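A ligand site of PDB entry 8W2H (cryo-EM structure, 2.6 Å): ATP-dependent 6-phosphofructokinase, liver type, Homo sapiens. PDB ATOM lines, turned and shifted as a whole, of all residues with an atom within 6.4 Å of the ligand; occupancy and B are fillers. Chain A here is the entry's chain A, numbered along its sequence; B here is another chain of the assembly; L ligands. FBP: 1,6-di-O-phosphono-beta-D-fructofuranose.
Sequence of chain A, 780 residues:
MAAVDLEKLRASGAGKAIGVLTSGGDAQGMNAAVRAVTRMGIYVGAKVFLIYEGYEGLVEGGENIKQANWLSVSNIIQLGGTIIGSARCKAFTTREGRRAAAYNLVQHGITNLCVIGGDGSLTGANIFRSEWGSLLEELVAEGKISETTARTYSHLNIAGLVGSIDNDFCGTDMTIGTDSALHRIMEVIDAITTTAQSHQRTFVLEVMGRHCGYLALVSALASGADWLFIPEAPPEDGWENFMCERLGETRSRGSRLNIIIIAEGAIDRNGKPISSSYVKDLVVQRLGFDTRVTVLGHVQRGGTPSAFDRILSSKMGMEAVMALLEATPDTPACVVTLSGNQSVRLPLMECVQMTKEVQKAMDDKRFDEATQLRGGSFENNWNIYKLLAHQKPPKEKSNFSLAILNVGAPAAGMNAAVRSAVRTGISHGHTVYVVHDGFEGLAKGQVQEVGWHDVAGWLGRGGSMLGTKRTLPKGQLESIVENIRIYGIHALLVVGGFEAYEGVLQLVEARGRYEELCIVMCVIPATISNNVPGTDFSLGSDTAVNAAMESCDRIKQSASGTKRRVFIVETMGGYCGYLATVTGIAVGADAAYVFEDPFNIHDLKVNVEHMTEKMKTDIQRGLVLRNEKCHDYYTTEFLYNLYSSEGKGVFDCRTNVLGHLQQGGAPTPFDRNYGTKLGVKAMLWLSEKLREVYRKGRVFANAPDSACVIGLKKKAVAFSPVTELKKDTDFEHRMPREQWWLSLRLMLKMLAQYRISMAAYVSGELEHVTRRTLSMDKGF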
ATOM      1  N   GLY A 408     -10.383  -6.048 -22.702  1.00  0.00           N
ATOM      2  CA  GLY A 408     -10.005  -6.113 -21.302  1.00  0.00           C
ATOM      3  C   GLY A 408     -11.196  -6.107 -20.368  1.00  0.00           C
ATOM      4  O   GLY A 408     -12.261  -6.606 -20.715  1.00  0.00           O
ATOM      5  N   ALA A 409     -11.010  -5.582 -19.154  1.00  0.00           N
ATOM      6  CA  ALA A 409     -12.137  -5.349 -18.271  1.00  0.00           C
ATOM      7  C   ALA A 409     -12.912  -4.111 -18.745  1.00  0.00           C
ATOM      8  O   ALA A 409     -12.334  -3.229 -19.382  1.00  0.00           O
ATOM      9  CB  ALA A 409     -11.659  -5.118 -16.843  1.00  0.00           C
ATOM     10  N   PRO A 410     -14.200  -4.007 -18.418  1.00  0.00           N
ATOM     11  CA  PRO A 410     -14.897  -2.749 -18.674  1.00  0.00           C
ATOM     12  C   PRO A 410     -14.334  -1.642 -17.806  1.00  0.00           C
ATOM     13  O   PRO A 410     -13.861  -1.883 -16.694  1.00  0.00           O
ATOM     14  CB  PRO A 410     -16.358  -3.054 -18.326  1.00  0.00           C
ATOM     15  CG  PRO A 410     -16.279  -4.188 -17.381  1.00  0.00           C
ATOM     16  CD  PRO A 410     -15.100  -4.998 -17.791  1.00  0.00           C
ATOM     17  N   ARG A 470     -11.047 -10.120 -22.458  1.00  0.00           N
ATOM     18  CA  ARG A 470      -9.611 -10.014 -22.209  1.00  0.00           C
ATOM     19  C   ARG A 470      -8.767 -10.814 -23.194  1.00  0.00           C
ATOM     20  O   ARG A 470      -7.540 -10.682 -23.142  1.00  0.00           O
ATOM     21  CB  ARG A 470      -9.290 -10.502 -20.796  1.00  0.00           C
ATOM     22  CG  ARG A 470      -9.824  -9.641 -19.680  1.00  0.00           C
ATOM     23  CD  ARG A 470      -9.500 -10.271 -18.345  1.00  0.00           C
ATOM     24  NE  ARG A 470     -10.017  -9.524 -17.213  1.00  0.00           N
ATOM     25  CZ  ARG A 470      -9.418  -8.476 -16.649  1.00  0.00           C
ATOM     26  NH1 ARG A 470      -8.304  -7.953 -17.144  1.00  0.00           N
ATOM     27  NH2 ARG A 470      -9.951  -7.957 -15.541  1.00  0.00           N
ATOM     28  N   GLY A 497      -7.643  -1.904 -21.605  1.00  0.00           N
ATOM     29  CA  GLY A 497      -6.566  -1.893 -20.631  1.00  0.00           C
ATOM     30  C   GLY A 497      -5.244  -2.449 -21.133  1.00  0.00           C
ATOM     31  O   GLY A 497      -4.864  -2.228 -22.282  1.00  0.00           O
ATOM     32  N   PHE A 498      -4.529  -3.161 -20.256  1.00  0.00           N
ATOM     33  CA  PHE A 498      -3.241  -3.715 -20.629  1.00  0.00           C
ATOM     34  C   PHE A 498      -3.359  -4.736 -21.748  1.00  0.00           C
ATOM     35  O   PHE A 498      -2.444  -4.869 -22.567  1.00  0.00           O
ATOM     36  CB  PHE A 498      -2.569  -4.346 -19.409  1.00  0.00           C
ATOM     37  CG  PHE A 498      -1.180  -4.822 -19.669  1.00  0.00           C
ATOM     38  CD1 PHE A 498      -0.117  -3.942 -19.620  1.00  0.00           C
ATOM     39  CD2 PHE A 498      -0.926  -6.153 -19.970  1.00  0.00           C
ATOM     40  CE1 PHE A 498       1.163  -4.363 -19.861  1.00  0.00           C
ATOM     41  CE2 PHE A 498       0.366  -6.583 -20.226  1.00  0.00           C
ATOM     42  CZ  PHE A 498       1.412  -5.686 -20.165  1.00  0.00           C
ATOM     43  N   GLU A 499      -4.478  -5.470 -21.802  1.00  0.00           N
ATOM     44  CA  GLU A 499      -4.670  -6.424 -22.886  1.00  0.00           C
ATOM     45  C   GLU A 499      -4.911  -5.727 -24.217  1.00  0.00           C
ATOM     46  O   GLU A 499      -4.631  -6.302 -25.280  1.00  0.00           O
ATOM     47  CB  GLU A 499      -5.833  -7.371 -22.564  1.00  0.00           C
ATOM     48  CG  GLU A 499      -5.835  -7.955 -21.150  1.00  0.00           C
ATOM     49  CD  GLU A 499      -4.499  -8.540 -20.743  1.00  0.00           C
ATOM     50  OE1 GLU A 499      -3.776  -9.060 -21.619  1.00  0.00           O
ATOM     51  OE2 GLU A 499      -4.179  -8.477 -19.540  1.00  0.00           O
ATOM     52  N   ALA A 526      -7.872   2.352 -21.293  1.00  0.00           N
ATOM     53  CA  ALA A 526      -9.103   2.463 -20.510  1.00  0.00           C
ATOM     54  C   ALA A 526      -9.122   1.328 -19.492  1.00  0.00           C
ATOM     55  O   ALA A 526      -9.466   0.197 -19.819  1.00  0.00           O
ATOM     56  CB  ALA A 526     -10.341   2.407 -21.405  1.00  0.00           C
ATOM     57  N   THR A 527      -8.759   1.648 -18.252  1.00  0.00           N
ATOM     58  CA  THR A 527      -8.755   0.623 -17.219  1.00  0.00           C
ATOM     59  C   THR A 527      -8.782   1.258 -15.840  1.00  0.00           C
ATOM     60  O   THR A 527      -8.335   2.399 -15.641  1.00  0.00           O
ATOM     61  CB  THR A 527      -7.554  -0.317 -17.349  1.00  0.00           C
ATOM     62  OG1 THR A 527      -7.620  -1.323 -16.330  1.00  0.00           O
ATOM     63  CG2 THR A 527      -6.233   0.415 -17.226  1.00  0.00           C
ATOM     64  N   ILE A 528      -9.315   0.494 -14.886  1.00  0.00           N
ATOM     65  CA  ILE A 528      -9.376   0.904 -13.497  1.00  0.00           C
ATOM     66  C   ILE A 528      -7.972   1.022 -12.916  1.00  0.00           C
ATOM     67  O   ILE A 528      -7.683   1.946 -12.141  1.00  0.00           O
ATOM     68  CB  ILE A 528     -10.237  -0.120 -12.712  1.00  0.00           C
ATOM     69  CG1 ILE A 528     -11.701  -0.119 -13.197  1.00  0.00           C
ATOM     70  CG2 ILE A 528     -10.129   0.067 -11.199  1.00  0.00           C
ATOM     71  CD1 ILE A 528     -12.520   1.117 -12.873  1.00  0.00           C
ATOM     72  N   SER A 529      -7.084   0.092 -13.273  1.00  0.00           N
ATOM     73  CA  SER A 529      -5.800  -0.028 -12.590  1.00  0.00           C
ATOM     74  C   SER A 529      -4.819   1.083 -12.949  1.00  0.00           C
ATOM     75  O   SER A 529      -3.874   1.320 -12.183  1.00  0.00           O
ATOM     76  CB  SER A 529      -5.191  -1.387 -12.922  1.00  0.00           C
ATOM     77  OG  SER A 529      -6.160  -2.414 -12.822  1.00  0.00           O
ATOM     78  N   ASN A 531      -2.754   0.838 -15.411  1.00  0.00           N
ATOM     79  CA  ASN A 531      -1.584  -0.019 -15.563  1.00  0.00           C
ATOM     80  C   ASN A 531      -1.117  -0.147 -17.014  1.00  0.00           C
ATOM     81  O   ASN A 531      -0.358  -1.070 -17.325  1.00  0.00           O
ATOM     82  CB  ASN A 531      -1.882  -1.412 -14.994  1.00  0.00           C
ATOM     83  CG  ASN A 531      -2.914  -2.157 -15.811  1.00  0.00           C
ATOM     84  OD1 ASN A 531      -3.714  -1.558 -16.509  1.00  0.00           O
ATOM     85  ND2 ASN A 531      -2.903  -3.478 -15.708  1.00  0.00           N
ATOM     86  N   VAL A 532      -1.554   0.729 -17.896  1.00  0.00           N
ATOM     87  CA  VAL A 532      -1.233   0.651 -19.323  1.00  0.00           C
ATOM     88  C   VAL A 532      -0.030   1.556 -19.588  1.00  0.00           C
ATOM     89  O   VAL A 532      -0.063   2.725 -19.197  1.00  0.00           O
ATOM     90  CB  VAL A 532      -2.420   1.056 -20.215  1.00  0.00           C
ATOM     91  CG1 VAL A 532      -2.052   0.904 -21.692  1.00  0.00           C
ATOM     92  CG2 VAL A 532      -3.642   0.225 -19.875  1.00  0.00           C
ATOM     93  N   MET A 572      -8.437  -2.707  -5.470  1.00  0.00           N
ATOM     94  CA  MET A 572      -8.085  -3.446  -6.676  1.00  0.00           C
ATOM     95  C   MET A 572      -6.915  -2.737  -7.370  1.00  0.00           C
ATOM     96  O   MET A 572      -6.284  -1.835  -6.801  1.00  0.00           O
ATOM     97  CB  MET A 572      -9.324  -3.582  -7.565  1.00  0.00           C
ATOM     98  CG  MET A 572     -10.322  -4.622  -7.073  1.00  0.00           C
ATOM     99  SD  MET A 572     -11.668  -5.003  -8.212  1.00  0.00           S
ATOM    100  CE  MET A 572     -12.237  -3.371  -8.701  1.00  0.00           C
ATOM    101  N   GLY A 573      -6.586  -3.163  -8.588  1.00  0.00           N
ATOM    102  CA  GLY A 573      -5.552  -2.567  -9.410  1.00  0.00           C
ATOM    103  C   GLY A 573      -4.459  -3.546  -9.806  1.00  0.00           C
ATOM    104  O   GLY A 573      -3.470  -3.138 -10.424  1.00  0.00           O
ATOM    105  N   GLY A 574      -4.628  -4.826  -9.483  1.00  0.00           N
ATOM    106  CA  GLY A 574      -3.594  -5.811  -9.773  1.00  0.00           C
ATOM    107  C   GLY A 574      -2.299  -5.483  -9.061  1.00  0.00           C
ATOM    108  O   GLY A 574      -2.285  -5.065  -7.904  1.00  0.00           O
ATOM    109  N   GLU A 628      -4.449  -5.269  -3.649  1.00  0.00           N
ATOM    110  CA  GLU A 628      -4.807  -6.684  -3.614  1.00  0.00           C
ATOM    111  C   GLU A 628      -3.618  -7.608  -3.853  1.00  0.00           C
ATOM    112  O   GLU A 628      -3.588  -8.723  -3.305  1.00  0.00           O
ATOM    113  CB  GLU A 628      -5.901  -6.972  -4.654  1.00  0.00           C
ATOM    114  CG  GLU A 628      -5.536  -6.586  -6.094  1.00  0.00           C
ATOM    115  CD  GLU A 628      -6.673  -6.802  -7.060  1.00  0.00           C
ATOM    116  OE1 GLU A 628      -7.727  -7.307  -6.636  1.00  0.00           O
ATOM    117  OE2 GLU A 628      -6.522  -6.456  -8.256  1.00  0.00           O
ATOM    118  N   LYS A 629      -2.638  -7.182  -4.645  1.00  0.00           N
ATOM    119  CA  LYS A 629      -1.478  -7.989  -5.019  1.00  0.00           C
ATOM    120  C   LYS A 629      -0.171  -7.336  -4.583  1.00  0.00           C
ATOM    121  O   LYS A 629       0.859  -7.454  -5.254  1.00  0.00           O
ATOM    122  CB  LYS A 629      -1.496  -8.257  -6.526  1.00  0.00           C
ATOM    123  CG  LYS A 629      -2.536  -9.275  -6.956  1.00  0.00           C
ATOM    124  CD  LYS A 629      -2.548  -9.493  -8.464  1.00  0.00           C
ATOM    125  CE  LYS A 629      -3.847 -10.117  -8.932  1.00  0.00           C
ATOM    126  NZ  LYS A 629      -4.914  -9.117  -9.211  1.00  0.00           N
ATOM    127  N   GLY A 659     -14.495  -4.802  -3.380  1.00  0.00           N
ATOM    128  CA  GLY A 659     -14.391  -5.605  -4.572  1.00  0.00           C
ATOM    129  C   GLY A 659     -14.747  -4.804  -5.801  1.00  0.00           C
ATOM    130  O   GLY A 659     -14.044  -3.864  -6.176  1.00  0.00           O
ATOM    131  N   HIS A 660     -15.859  -5.167  -6.440  1.00  0.00           N
ATOM    132  CA  HIS A 660     -16.357  -4.465  -7.610  1.00  0.00           C
ATOM    133  C   HIS A 660     -17.157  -3.213  -7.266  1.00  0.00           C
ATOM    134  O   HIS A 660     -17.848  -2.675  -8.140  1.00  0.00           O
ATOM    135  CB  HIS A 660     -17.176  -5.429  -8.461  1.00  0.00           C
ATOM    136  CG  HIS A 660     -16.390  -6.605  -8.942  1.00  0.00           C
ATOM    137  ND1 HIS A 660     -16.044  -7.652  -8.116  1.00  0.00           N
ATOM    138  CD2 HIS A 660     -15.852  -6.886 -10.154  1.00  0.00           C
ATOM    139  CE1 HIS A 660     -15.345  -8.533  -8.808  1.00  0.00           C
ATOM    140  NE2 HIS A 660     -15.213  -8.093 -10.044  1.00  0.00           N
ATOM    141  N   GLN A 663     -15.683  -0.475  -9.552  1.00  0.00           N
ATOM    142  CA  GLN A 663     -15.653  -0.795 -10.974  1.00  0.00           C
ATOM    143  C   GLN A 663     -16.869  -0.266 -11.732  1.00  0.00           C
ATOM    144  O   GLN A 663     -16.719   0.533 -12.659  1.00  0.00           O
ATOM    145  CB  GLN A 663     -15.547  -2.331 -11.133  1.00  0.00           C
ATOM    146  CG  GLN A 663     -15.620  -2.872 -12.569  1.00  0.00           C
ATOM    147  CD  GLN A 663     -14.644  -2.211 -13.527  1.00  0.00           C
ATOM    148  OE1 GLN A 663     -14.758  -1.022 -13.830  1.00  0.00           O
ATOM    149  NE2 GLN A 663     -13.688  -2.990 -14.029  1.00  0.00           N
ATOM    150  N   ARG A 734       1.912  -7.045 -15.742  1.00  0.00           N
ATOM    151  CA  ARG A 734       0.944  -6.283 -16.537  1.00  0.00           C
ATOM    152  C   ARG A 734       0.883  -4.824 -16.114  1.00  0.00           C
ATOM    153  O   ARG A 734      -0.186  -4.267 -15.855  1.00  0.00           O
ATOM    154  CB  ARG A 734      -0.443  -6.928 -16.475  1.00  0.00           C
ATOM    155  CG  ARG A 734      -0.483  -8.376 -16.917  1.00  0.00           C
ATOM    156  CD  ARG A 734      -1.895  -8.842 -17.229  1.00  0.00           C
ATOM    157  NE  ARG A 734      -2.836  -8.467 -16.172  1.00  0.00           N
ATOM    158  CZ  ARG A 734      -3.813  -7.564 -16.252  1.00  0.00           C
ATOM    159  NH1 ARG A 734      -4.125  -6.940 -17.378  1.00  0.00           N
ATOM    160  NH2 ARG A 734      -4.503  -7.269 -15.151  1.00  0.00           N
ATOM    161  N   LYS B 563     -21.250 -10.696 -19.910  1.00  0.00           N
ATOM    162  CA  LYS B 563     -20.739 -11.521 -18.814  1.00  0.00           C
ATOM    163  C   LYS B 563     -21.854 -11.929 -17.867  1.00  0.00           C
ATOM    164  O   LYS B 563     -22.586 -11.083 -17.334  1.00  0.00           O
ATOM    165  CB  LYS B 563     -19.647 -10.796 -18.043  1.00  0.00           C
ATOM    166  CG  LYS B 563     -18.933 -11.731 -17.061  1.00  0.00           C
ATOM    167  CD  LYS B 563     -17.674 -11.139 -16.487  1.00  0.00           C
ATOM    168  CE  LYS B 563     -16.950 -12.172 -15.639  1.00  0.00           C
ATOM    169  NZ  LYS B 563     -16.281 -13.228 -16.458  1.00  0.00           N
ATOM    170  N   ARG B 565     -22.633 -13.246 -14.366  1.00  0.00           N
ATOM    171  CA  ARG B 565     -21.993 -13.312 -13.058  1.00  0.00           C
ATOM    172  C   ARG B 565     -22.990 -13.117 -11.926  1.00  0.00           C
ATOM    173  O   ARG B 565     -23.872 -12.253 -11.988  1.00  0.00           O
ATOM    174  CB  ARG B 565     -20.821 -12.322 -12.985  1.00  0.00           C
ATOM    175  CG  ARG B 565     -20.288 -11.951 -11.573  1.00  0.00           C
ATOM    176  CD  ARG B 565     -18.798 -12.063 -11.460  1.00  0.00           C
ATOM    177  NE  ARG B 565     -18.076 -10.929 -12.020  1.00  0.00           N
ATOM    178  CZ  ARG B 565     -16.806 -10.946 -12.407  1.00  0.00           C
ATOM    179  NH1 ARG B 565     -16.094 -12.067 -12.469  1.00  0.00           N
ATOM    180  NH2 ARG B 565     -16.221  -9.797 -12.746  1.00  0.00           N
ATOM    181  N   ASP B 652     -19.835 -16.937 -13.639  1.00  0.00           N
ATOM    182  CA  ASP B 652     -18.790 -16.693 -12.654  1.00  0.00           C
ATOM    183  C   ASP B 652     -19.428 -16.201 -11.362  1.00  0.00           C
ATOM    184  O   ASP B 652     -20.572 -15.729 -11.349  1.00  0.00           O
ATOM    185  CB  ASP B 652     -17.805 -15.668 -13.207  1.00  0.00           C
ATOM    186  CG  ASP B 652     -16.528 -15.574 -12.397  1.00  0.00           C
ATOM    187  OD1 ASP B 652     -16.227 -16.506 -11.613  1.00  0.00           O
ATOM    188  OD2 ASP B 652     -15.814 -14.561 -12.536  1.00  0.00           O
ATOM    189  N   ARG B 654     -18.632 -13.960  -7.605  1.00  0.00           N
ATOM    190  CA  ARG B 654     -17.790 -13.048  -6.840  1.00  0.00           C
ATOM    191  C   ARG B 654     -18.445 -12.751  -5.508  1.00  0.00           C
ATOM    192  O   ARG B 654     -19.637 -13.000  -5.297  1.00  0.00           O
ATOM    193  CB  ARG B 654     -17.520 -11.748  -7.608  1.00  0.00           C
ATOM    194  CG  ARG B 654     -16.530 -11.882  -8.759  1.00  0.00           C
ATOM    195  CD  ARG B 654     -15.103 -12.121  -8.297  1.00  0.00           C
ATOM    196  NE  ARG B 654     -14.215 -12.229  -9.457  1.00  0.00           N
ATOM    197  CZ  ARG B 654     -14.112 -13.285 -10.248  1.00  0.00           C
ATOM    198  NH1 ARG B 654     -14.825 -14.389 -10.034  1.00  0.00           N
ATOM    199  NH2 ARG B 654     -13.291 -13.245 -11.284  1.00  0.00           N
HETATM  200  P1  FBP L   1     -12.157  -9.894 -11.843  1.00  0.00           P
HETATM  201  O1P FBP L   1     -12.971 -10.409 -12.938  1.00  0.00           O
HETATM  202  O2P FBP L   1     -13.105  -9.635 -10.770  1.00  0.00           O
HETATM  203  O3P FBP L   1     -11.393 -11.048 -11.381  1.00  0.00           O
HETATM  204  O1  FBP L   1     -11.232  -8.592 -12.245  1.00  0.00           O
HETATM  205  C1  FBP L   1     -10.549  -7.932 -11.216  1.00  0.00           C
HETATM  206  C2  FBP L   1      -9.456  -7.020 -11.784  1.00  0.00           C
HETATM  207  O2  FBP L   1      -8.272  -7.699 -11.807  1.00  0.00           O
HETATM  208  C3  FBP L   1      -9.319  -5.792 -10.951  1.00  0.00           C
HETATM  209  O3  FBP L   1      -7.954  -5.341 -10.965  1.00  0.00           O
HETATM  210  C4  FBP L   1     -10.214  -4.800 -11.592  1.00  0.00           C
HETATM  211  O4  FBP L   1     -11.555  -4.931 -11.116  1.00  0.00           O
HETATM  212  C5  FBP L   1     -10.171  -5.122 -13.041  1.00  0.00           C
HETATM  213  O5  FBP L   1      -9.799  -6.545 -13.129  1.00  0.00           O
HETATM  214  C6  FBP L   1      -9.170  -4.234 -13.711  1.00  0.00           C
HETATM  215  O6  FBP L   1      -8.828  -4.727 -14.973  1.00  0.00           O
HETATM  216  P2  FBP L   1      -7.241  -4.893 -15.414  1.00  0.00           P
HETATM  217  O4P FBP L   1      -6.903  -6.237 -15.851  1.00  0.00           O
HETATM  218  O5P FBP L   1      -6.852  -4.048 -16.537  1.00  0.00           O
HETATM  219  O6P FBP L   1      -6.241  -4.610 -14.387  1.00  0.00           O
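NE2 of His 660 lies within hydrogen-bond range of O2P of the ligand, 2.7 Å away.
An oxygen (O4P) of the ligand lies within salt-bridge range of the guanidinium group (NH2) of Arg 734, 2.7 Å away.
O1P of the ligand is in salt-bridge range of NH2 of Arg 565 of chain B, at 3.3 Å.
O4 of the ligand sits at hydrogen-bond distance from SD of Met 572.
OG1 of Thr 527 is in hydrogen-bond range of O5P of the ligand, at 2.8 Å.
OG of Ser 529 is in hydrogen-bond range of O6P of the ligand (2.7 Å).
The guanidinium group (NH1) of Arg 470 is in salt-bridge range of an oxygen (O4P) of the ligand (2.6 Å).
The side-chain carboxylate of Glu 628 sits at hydrogen-bond distance from an oxygen (O3) of the ligand (3.3 Å).
O3P of the ligand lies within salt-bridge range of NH2 of Arg 654 of chain B (2.9 Å).
NH1 of Arg 734 is in salt-bridge range of OE2 of Glu 499, 2.7 Å away.
The backbone carbonyl oxygen of Arg 734 is in hydrogen-bond range of the side-chain amide nitrogen of Asn 531 (2.8 Å).
The guanidinium group (NH1) of Arg 654 of chain B is in salt-bridge range of the side-chain carboxylate (OD2) of Asp 652 of chain B.
NZ of Lys 629 lies within salt-bridge range of OE2 of Glu 628 (3.3 Å).
The guanidinium group (NH1) of Arg 565 of chain B lies within salt-bridge range of the side-chain carboxylate (OD2) of Asp 652 of chain B, 2.5 Å away.
OE2 of Glu 628 lies within hydrogen-bond range of N of Gly 573 (3.3 Å).
The backbone NH of Gly 574 sits at hydrogen-bond distance from the side-chain carboxylate of Glu 628, 2.8 Å away.
The backbone NH (N) of Ser 529 lies close to the side-chain hydroxyl (OG1) of Thr 527, 3.4 Å away.
Residues that only touch the ligand: Ala 409 (3.4 Å), Gly 573 (3.5 Å), Gly 574 (3.7 Å) and Asn 531 (3.8 Å).
Of the 26 residues printed, 13 come within 4 Å of the ligand.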
